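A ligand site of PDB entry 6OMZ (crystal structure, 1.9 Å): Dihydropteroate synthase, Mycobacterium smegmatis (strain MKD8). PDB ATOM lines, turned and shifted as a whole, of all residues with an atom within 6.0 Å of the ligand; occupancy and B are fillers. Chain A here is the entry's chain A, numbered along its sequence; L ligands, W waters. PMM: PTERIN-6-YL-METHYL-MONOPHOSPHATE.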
ATOM      1  N   MET A  25      -5.047 -21.230 -19.914  1.00  0.00           N
ATOM      2  CA  MET A  25      -6.478 -21.513 -20.048  1.00  0.00           C
ATOM      3  C   MET A  25      -6.894 -21.205 -21.484  1.00  0.00           C
ATOM      4  O   MET A  25      -6.940 -20.035 -21.879  1.00  0.00           O
ATOM      5  CB  MET A  25      -7.268 -20.672 -19.038  1.00  0.00           C
ATOM      6  CG  MET A  25      -8.771 -20.768 -19.168  1.00  0.00           C
ATOM      7  SD  MET A  25      -9.602 -19.567 -18.107  1.00  0.00           S
ATOM      8  CE  MET A  25      -9.411 -20.337 -16.490  1.00  0.00           C
ATOM      9  N   VAL A  27      -9.664 -21.033 -24.569  1.00  0.00           N
ATOM     10  CA  VAL A  27     -11.065 -20.648 -24.643  1.00  0.00           C
ATOM     11  C   VAL A  27     -11.775 -21.484 -25.709  1.00  0.00           C
ATOM     12  O   VAL A  27     -11.330 -21.540 -26.859  1.00  0.00           O
ATOM     13  CB  VAL A  27     -11.212 -19.147 -24.957  1.00  0.00           C
ATOM     14  CG1 VAL A  27     -12.691 -18.781 -25.195  1.00  0.00           C
ATOM     15  CG2 VAL A  27     -10.663 -18.316 -23.838  1.00  0.00           C
ATOM     16  N   ASP A  63     -11.625 -23.353 -20.921  1.00  0.00           N
ATOM     17  CA  ASP A  63     -12.693 -22.475 -20.456  1.00  0.00           C
ATOM     18  C   ASP A  63     -13.828 -22.532 -21.476  1.00  0.00           C
ATOM     19  O   ASP A  63     -13.701 -21.986 -22.583  1.00  0.00           O
ATOM     20  CB  ASP A  63     -12.156 -21.050 -20.278  1.00  0.00           C
ATOM     21  CG  ASP A  63     -13.189 -20.084 -19.695  1.00  0.00           C
ATOM     22  OD1 ASP A  63     -13.821 -20.417 -18.665  1.00  0.00           O
ATOM     23  OD2 ASP A  63     -13.342 -18.978 -20.248  1.00  0.00           O
ATOM     24  N   THR A  69     -20.742 -11.289 -23.952  1.00  0.00           N
ATOM     25  CA  THR A  69     -21.212 -10.095 -23.258  1.00  0.00           C
ATOM     26  C   THR A  69     -20.972  -8.826 -24.049  1.00  0.00           C
ATOM     27  O   THR A  69     -21.365  -7.760 -23.580  1.00  0.00           O
ATOM     28  CB  THR A  69     -20.532  -9.958 -21.889  1.00  0.00           C
ATOM     29  OG1 THR A  69     -19.112 -10.053 -22.080  1.00  0.00           O
ATOM     30  CG2 THR A  69     -21.011 -11.037 -20.923  1.00  0.00           C
ATOM     31  N   ARG A  70     -20.353  -8.891 -25.219  1.00  0.00           N
ATOM     32  CA  ARG A  70     -19.990  -7.668 -25.920  1.00  0.00           C
ATOM     33  C   ARG A  70     -21.226  -6.986 -26.515  1.00  0.00           C
ATOM     34  O   ARG A  70     -22.258  -7.637 -26.738  1.00  0.00           O
ATOM     35  CB  ARG A  70     -18.962  -7.967 -27.001  1.00  0.00           C
ATOM     36  CG  ARG A  70     -19.417  -8.865 -28.114  1.00  0.00           C
ATOM     37  CD  ARG A  70     -18.259  -9.085 -29.078  1.00  0.00           C
ATOM     38  NE  ARG A  70     -17.025  -9.289 -28.323  1.00  0.00           N
ATOM     39  CZ  ARG A  70     -16.537 -10.489 -28.002  1.00  0.00           C
ATOM     40  NH1 ARG A  70     -17.164 -11.579 -28.412  1.00  0.00           N
ATOM     41  NH2 ARG A  70     -15.431 -10.594 -27.269  1.00  0.00           N
ATOM     42  N   ASP A 102     -17.487 -20.580 -18.180  1.00  0.00           N
ATOM     43  CA  ASP A 102     -17.524 -19.118 -18.271  1.00  0.00           C
ATOM     44  C   ASP A 102     -18.996 -18.718 -18.289  1.00  0.00           C
ATOM     45  O   ASP A 102     -19.645 -18.725 -19.338  1.00  0.00           O
ATOM     46  CB  ASP A 102     -16.777 -18.654 -19.520  1.00  0.00           C
ATOM     47  CG  ASP A 102     -16.668 -17.144 -19.645  1.00  0.00           C
ATOM     48  OD1 ASP A 102     -17.432 -16.390 -18.987  1.00  0.00           O
ATOM     49  OD2 ASP A 102     -15.797 -16.692 -20.416  1.00  0.00           O
ATOM     50  N   ASN A 121     -15.985 -19.617 -13.863  1.00  0.00           N
ATOM     51  CA  ASN A 121     -15.366 -18.367 -14.298  1.00  0.00           C
ATOM     52  C   ASN A 121     -16.462 -17.325 -14.515  1.00  0.00           C
ATOM     53  O   ASN A 121     -17.187 -17.378 -15.510  1.00  0.00           O
ATOM     54  CB  ASN A 121     -14.570 -18.589 -15.596  1.00  0.00           C
ATOM     55  CG  ASN A 121     -13.978 -17.309 -16.132  1.00  0.00           C
ATOM     56  OD1 ASN A 121     -13.709 -16.385 -15.374  1.00  0.00           O
ATOM     57  ND2 ASN A 121     -13.770 -17.246 -17.450  1.00  0.00           N
ATOM     58  N   ASP A 122     -16.577 -16.369 -13.585  1.00  0.00           N
ATOM     59  CA  ASP A 122     -17.708 -15.435 -13.538  1.00  0.00           C
ATOM     60  C   ASP A 122     -17.240 -14.024 -13.884  1.00  0.00           C
ATOM     61  O   ASP A 122     -16.636 -13.350 -13.040  1.00  0.00           O
ATOM     62  CB  ASP A 122     -18.324 -15.494 -12.144  1.00  0.00           C
ATOM     63  CG  ASP A 122     -19.581 -14.646 -12.003  1.00  0.00           C
ATOM     64  OD1 ASP A 122     -19.977 -13.901 -12.939  1.00  0.00           O
ATOM     65  OD2 ASP A 122     -20.169 -14.739 -10.908  1.00  0.00           O
ATOM     66  N   VAL A 123     -17.525 -13.570 -15.106  1.00  0.00           N
ATOM     67  CA  VAL A 123     -17.072 -12.231 -15.504  1.00  0.00           C
ATOM     68  C   VAL A 123     -17.769 -11.136 -14.693  1.00  0.00           C
ATOM     69  O   VAL A 123     -17.299  -9.988 -14.688  1.00  0.00           O
ATOM     70  CB  VAL A 123     -17.231 -11.982 -17.024  1.00  0.00           C
ATOM     71  CG1 VAL A 123     -16.427 -13.029 -17.836  1.00  0.00           C
ATOM     72  CG2 VAL A 123     -18.701 -11.960 -17.443  1.00  0.00           C
ATOM     73  N   ILE A 144     -13.436 -18.072 -10.050  1.00  0.00           N
ATOM     74  CA  ILE A 144     -12.713 -16.932 -10.589  1.00  0.00           C
ATOM     75  C   ILE A 144     -13.637 -15.729 -10.572  1.00  0.00           C
ATOM     76  O   ILE A 144     -14.698 -15.731 -11.214  1.00  0.00           O
ATOM     77  CB  ILE A 144     -12.228 -17.211 -12.032  1.00  0.00           C
ATOM     78  CG1 ILE A 144     -11.264 -18.404 -12.062  1.00  0.00           C
ATOM     79  CG2 ILE A 144     -11.545 -15.971 -12.628  1.00  0.00           C
ATOM     80  CD1 ILE A 144     -11.055 -19.004 -13.470  1.00  0.00           C
ATOM     81  N   MET A 146     -13.927 -12.051 -11.765  1.00  0.00           N
ATOM     82  CA  MET A 146     -13.403 -11.021 -12.646  1.00  0.00           C
ATOM     83  C   MET A 146     -13.955  -9.644 -12.270  1.00  0.00           C
ATOM     84  O   MET A 146     -15.096  -9.511 -11.841  1.00  0.00           O
ATOM     85  CB  MET A 146     -13.752 -11.309 -14.110  1.00  0.00           C
ATOM     86  CG  MET A 146     -12.805 -10.624 -15.087  1.00  0.00           C
ATOM     87  SD  MET A 146     -13.468 -10.563 -16.773  1.00  0.00           S
ATOM     88  CE  MET A 146     -14.667  -9.231 -16.566  1.00  0.00           C
ATOM     89  N   ASP A 193      -9.282 -11.603 -11.180  1.00  0.00           N
ATOM     90  CA  ASP A 193      -8.931 -11.268 -12.577  1.00  0.00           C
ATOM     91  C   ASP A 193      -9.245  -9.781 -12.727  1.00  0.00           C
ATOM     92  O   ASP A 193     -10.377  -9.385 -12.420  1.00  0.00           O
ATOM     93  CB  ASP A 193      -9.743 -12.131 -13.557  1.00  0.00           C
ATOM     94  CG  ASP A 193      -9.417 -11.867 -15.036  1.00  0.00           C
ATOM     95  OD1 ASP A 193      -9.082 -10.734 -15.412  1.00  0.00           O
ATOM     96  OD2 ASP A 193      -9.541 -12.834 -15.834  1.00  0.00           O
ATOM     97  N   GLY A 195     -10.028  -8.070 -15.212  1.00  0.00           N
ATOM     98  CA  GLY A 195     -11.057  -7.782 -16.195  1.00  0.00           C
ATOM     99  C   GLY A 195     -10.626  -6.748 -17.216  1.00  0.00           C
ATOM    100  O   GLY A 195     -11.308  -5.738 -17.398  1.00  0.00           O
ATOM    101  N   LEU A 196      -9.495  -6.996 -17.898  1.00  0.00           N
ATOM    102  CA  LEU A 196      -8.983  -6.024 -18.849  1.00  0.00           C
ATOM    103  C   LEU A 196     -10.021  -5.707 -19.919  1.00  0.00           C
ATOM    104  O   LEU A 196     -10.686  -6.609 -20.449  1.00  0.00           O
ATOM    105  CB  LEU A 196      -7.699  -6.563 -19.499  1.00  0.00           C
ATOM    106  CG  LEU A 196      -6.562  -6.982 -18.567  1.00  0.00           C
ATOM    107  CD1 LEU A 196      -5.406  -7.597 -19.373  1.00  0.00           C
ATOM    108  CD2 LEU A 196      -6.078  -5.775 -17.765  1.00  0.00           C
ATOM    109  N   PHE A 198     -12.963  -4.487 -19.743  1.00  0.00           N
ATOM    110  CA  PHE A 198     -14.367  -4.465 -19.316  1.00  0.00           C
ATOM    111  C   PHE A 198     -14.627  -3.136 -18.600  1.00  0.00           C
ATOM    112  O   PHE A 198     -14.269  -2.970 -17.432  1.00  0.00           O
ATOM    113  CB  PHE A 198     -14.674  -5.649 -18.410  1.00  0.00           C
ATOM    114  CG  PHE A 198     -14.840  -6.955 -19.140  1.00  0.00           C
ATOM    115  CD1 PHE A 198     -13.743  -7.730 -19.464  1.00  0.00           C
ATOM    116  CD2 PHE A 198     -16.114  -7.412 -19.469  1.00  0.00           C
ATOM    117  CE1 PHE A 198     -13.904  -8.941 -20.109  1.00  0.00           C
ATOM    118  CE2 PHE A 198     -16.283  -8.633 -20.118  1.00  0.00           C
ATOM    119  CZ  PHE A 198     -15.171  -9.398 -20.453  1.00  0.00           C
ATOM    120  N   LEU A 223      -5.609 -14.396 -12.496  1.00  0.00           N
ATOM    121  CA  LEU A 223      -5.767 -14.764 -13.896  1.00  0.00           C
ATOM    122  C   LEU A 223      -5.816 -13.495 -14.733  1.00  0.00           C
ATOM    123  O   LEU A 223      -6.459 -12.518 -14.349  1.00  0.00           O
ATOM    124  CB  LEU A 223      -7.064 -15.556 -14.109  1.00  0.00           C
ATOM    125  CG  LEU A 223      -7.522 -15.894 -15.535  1.00  0.00           C
ATOM    126  CD1 LEU A 223      -6.551 -16.860 -16.191  1.00  0.00           C
ATOM    127  CD2 LEU A 223      -8.942 -16.480 -15.511  1.00  0.00           C
ATOM    128  N   VAL A 224      -5.125 -13.503 -15.876  1.00  0.00           N
ATOM    129  CA  VAL A 224      -5.085 -12.359 -16.791  1.00  0.00           C
ATOM    130  C   VAL A 224      -5.750 -12.761 -18.110  1.00  0.00           C
ATOM    131  O   VAL A 224      -5.401 -13.797 -18.694  1.00  0.00           O
ATOM    132  CB  VAL A 224      -3.638 -11.895 -17.051  1.00  0.00           C
ATOM    133  CG1 VAL A 224      -3.592 -10.873 -18.156  1.00  0.00           C
ATOM    134  CG2 VAL A 224      -3.028 -11.351 -15.771  1.00  0.00           C
ATOM    135  N   GLY A 225      -6.677 -11.936 -18.586  1.00  0.00           N
ATOM    136  CA  GLY A 225      -7.247 -12.160 -19.904  1.00  0.00           C
ATOM    137  C   GLY A 225      -7.076 -10.968 -20.823  1.00  0.00           C
ATOM    138  O   GLY A 225      -7.852 -10.006 -20.775  1.00  0.00           O
ATOM    139  N   ALA A 226      -6.034 -10.995 -21.655  1.00  0.00           N
ATOM    140  CA  ALA A 226      -5.783  -9.910 -22.606  1.00  0.00           C
ATOM    141  C   ALA A 226      -6.078 -10.297 -24.045  1.00  0.00           C
ATOM    142  O   ALA A 226      -6.151  -9.420 -24.912  1.00  0.00           O
ATOM    143  CB  ALA A 226      -4.337  -9.439 -22.503  1.00  0.00           C
ATOM    144  N   SER A 227      -6.277 -11.578 -24.319  1.00  0.00           N
ATOM    145  CA  SER A 227      -6.253 -12.151 -25.659  1.00  0.00           C
ATOM    146  C   SER A 227      -7.169 -11.407 -26.621  1.00  0.00           C
ATOM    147  O   SER A 227      -8.389 -11.385 -26.433  1.00  0.00           O
ATOM    148  CB  SER A 227      -6.637 -13.625 -25.574  1.00  0.00           C
ATOM    149  OG  SER A 227      -6.643 -14.230 -26.865  1.00  0.00           O
ATOM    150  N   ARG A 228      -6.577 -10.812 -27.663  1.00  0.00           N
ATOM    151  CA  ARG A 228      -7.281 -10.180 -28.774  1.00  0.00           C
ATOM    152  C   ARG A 228      -8.125  -8.984 -28.351  1.00  0.00           C
ATOM    153  O   ARG A 228      -8.927  -8.503 -29.152  1.00  0.00           O
ATOM    154  CB  ARG A 228      -8.162 -11.193 -29.506  1.00  0.00           C
ATOM    155  CG  ARG A 228      -7.382 -12.418 -29.992  1.00  0.00           C
ATOM    156  CD  ARG A 228      -8.310 -13.536 -30.466  1.00  0.00           C
ATOM    157  NE  ARG A 228      -9.108 -13.187 -31.629  1.00  0.00           N
ATOM    158  CZ  ARG A 228      -8.759 -13.446 -32.887  1.00  0.00           C
ATOM    159  NH1 ARG A 228      -7.602 -14.050 -33.144  1.00  0.00           N
ATOM    160  NH2 ARG A 228      -9.560 -13.111 -33.879  1.00  0.00           N
ATOM    161  N   LYS A 229      -7.960  -8.476 -27.138  1.00  0.00           N
ATOM    162  CA  LYS A 229      -8.834  -7.414 -26.646  1.00  0.00           C
ATOM    163  C   LYS A 229      -8.584  -6.097 -27.387  1.00  0.00           C
ATOM    164  O   LYS A 229      -7.551  -5.892 -28.038  1.00  0.00           O
ATOM    165  CB  LYS A 229      -8.646  -7.238 -25.143  1.00  0.00           C
ATOM    166  CG  LYS A 229      -9.105  -8.452 -24.334  1.00  0.00           C
ATOM    167  CD  LYS A 229     -10.110  -8.073 -23.267  1.00  0.00           C
ATOM    168  CE  LYS A 229     -10.702  -9.295 -22.584  1.00  0.00           C
ATOM    169  NZ  LYS A 229     -10.392  -9.336 -21.139  1.00  0.00           N
ATOM    170  N   ARG A 269      -5.685 -16.441 -19.794  1.00  0.00           N
ATOM    171  CA  ARG A 269      -6.824 -16.916 -20.589  1.00  0.00           C
ATOM    172  C   ARG A 269      -6.610 -16.465 -22.030  1.00  0.00           C
ATOM    173  O   ARG A 269      -6.531 -15.262 -22.303  1.00  0.00           O
ATOM    174  CB  ARG A 269      -8.141 -16.368 -20.018  1.00  0.00           C
ATOM    175  CG  ARG A 269      -9.403 -16.883 -20.724  1.00  0.00           C
ATOM    176  CD  ARG A 269     -10.670 -16.213 -20.135  1.00  0.00           C
ATOM    177  NE  ARG A 269     -11.885 -16.634 -20.812  1.00  0.00           N
ATOM    178  CZ  ARG A 269     -12.368 -16.083 -21.923  1.00  0.00           C
ATOM    179  NH1 ARG A 269     -11.729 -15.070 -22.495  1.00  0.00           N
ATOM    180  NH2 ARG A 269     -13.490 -16.524 -22.467  1.00  0.00           N
ATOM    181  N   HIS A 271      -7.076 -17.394 -26.526  1.00  0.00           N
ATOM    182  CA  HIS A 271      -7.644 -18.153 -27.621  1.00  0.00           C
ATOM    183  C   HIS A 271      -6.569 -18.969 -28.344  1.00  0.00           C
ATOM    184  O   HIS A 271      -6.792 -20.140 -28.686  1.00  0.00           O
ATOM    185  CB  HIS A 271      -8.328 -17.198 -28.608  1.00  0.00           C
ATOM    186  CG  HIS A 271      -9.471 -16.443 -28.006  1.00  0.00           C
ATOM    187  ND1 HIS A 271     -10.765 -16.914 -28.026  1.00  0.00           N
ATOM    188  CD2 HIS A 271      -9.506 -15.248 -27.358  1.00  0.00           C
ATOM    189  CE1 HIS A 271     -11.560 -16.029 -27.427  1.00  0.00           C
ATOM    190  NE2 HIS A 271     -10.823 -15.023 -27.004  1.00  0.00           N
HETATM  191  N5  PMM L   1     -12.822 -12.137 -21.241  1.00  0.00           N
HETATM  192  C6  PMM L   1     -13.913 -12.596 -21.879  1.00  0.00           C
HETATM  193  C7  PMM L   1     -14.652 -13.646 -21.347  1.00  0.00           C
HETATM  194  N8  PMM L   1     -14.387 -14.249 -20.186  1.00  0.00           N
HETATM  195  N1  PMM L   1     -13.081 -14.348 -18.327  1.00  0.00           N
HETATM  196  C2  PMM L   1     -12.059 -13.905 -17.600  1.00  0.00           C
HETATM  197  N2  PMM L   1     -11.833 -14.418 -16.399  1.00  0.00           N
HETATM  198  N3  PMM L   1     -11.229 -12.901 -18.025  1.00  0.00           N
HETATM  199  C4  PMM L   1     -11.348 -12.229 -19.227  1.00  0.00           C
HETATM  200  O4  PMM L   1     -10.545 -11.359 -19.538  1.00  0.00           O
HETATM  201  C4A PMM L   1     -12.482 -12.676 -20.057  1.00  0.00           C
HETATM  202  C8A PMM L   1     -13.312 -13.758 -19.549  1.00  0.00           C
HETATM  203  C9  PMM L   1     -14.337 -11.858 -23.115  1.00  0.00           C
HETATM  204  O10 PMM L   1     -13.381 -12.087 -24.179  1.00  0.00           O
HETATM  205  PA  PMM L   1     -13.442 -13.235 -25.331  1.00  0.00           P
HETATM  206  O1P PMM L   1     -12.200 -13.060 -26.121  1.00  0.00           O
HETATM  207  O2P PMM L   1     -13.496 -14.613 -24.665  1.00  0.00           O
HETATM  208  O3P PMM L   1     -14.704 -13.019 -26.156  1.00  0.00           O
HETATM  209  O   HOH W   1     -17.705 -12.229 -21.643  1.00  0.00           O
HETATM  210  O   HOH W   2      -9.956 -12.196 -24.427  1.00  0.00           O
HETATM  211  O   HOH W   3      -8.703  -9.893 -17.827  1.00  0.00           O
HETATM  212  O   HOH W   4     -17.151 -13.599 -25.478  1.00  0.00           O
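A ring nitrogen (NE2) of His 271 lies within hydrogen-bond range of an oxygen (O1P) of the ligand, at 2.6 Å.
The side-chain amino group of Lys 229 lies within hydrogen-bond range of an oxygen (O4) of the ligand.
An oxygen (O3P) of the ligand lies within salt-bridge range of the guanidinium group (NH2) of Arg 70.
The side-chain carboxylate of Asp 193 sits at hydrogen-bond distance from a nitrogen (N3) of the ligand.
OD2 of Asp 102 lies within hydrogen-bond range of N8 of the ligand.
The guanidinium group (NH1) of Arg 269 is in salt-bridge range of an oxygen (O2P) of the ligand.
The side-chain amide oxygen of Asn 121 is in hydrogen-bond range of a nitrogen (N2) of the ligand (2.9 Å).
The side-chain sulfur (SD) of Met 146 sits at hydrogen-bond distance from a nitrogen (N3) of the ligand.
The backbone NH (N) of His 271 sits close to the side-chain hydroxyl (OG) of Ser 227 (3.2 Å).
The side-chain amino group (NZ) of Lys 229 sits at hydrogen-bond distance from the backbone carbonyl oxygen (O) of Gly 225.
The backbone carbonyl oxygen (O) of Leu 196 is in hydrogen-bond range of the side-chain amino group (NZ) of Lys 229, 2.8 Å away.
OD1 of Asp 193 lies within hydrogen-bond range of N of Gly 195 (2.8 Å).
OD2 of Asp 102 is in salt-bridge range of NH2 of Arg 269, 3.1 Å away.
The side-chain carboxylate (OD2) of Asp 63 is in salt-bridge range of the guanidinium group (NE) of Arg 269, 2.8 Å away.
The backbone carbonyl oxygen (O) of Val 224 sits at hydrogen-bond distance from the backbone NH (N) of Arg 269 (2.9 Å).
The side-chain amide nitrogen (ND2) of Asn 121 lies within hydrogen-bond range of the side-chain carboxylate (OD2) of Asp 63 (3.3 Å).
The backbone carbonyl oxygen (O) of Gly 225 lies close to an oxygen (O4) of the ligand, at 3.3 Å.
Merely in contact with the ligand: Val 123 (3.3 Å), Phe 198 (3.6 Å) and Leu 223 (3.7 Å).
The nearest printed residue that does not touch the ligand is Ile 144 (4.1 Å).
Water W2 lies within hydrogen-bond range of O of Ser 227 (2.7 Å) and O1P of the ligand (2.9 Å).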
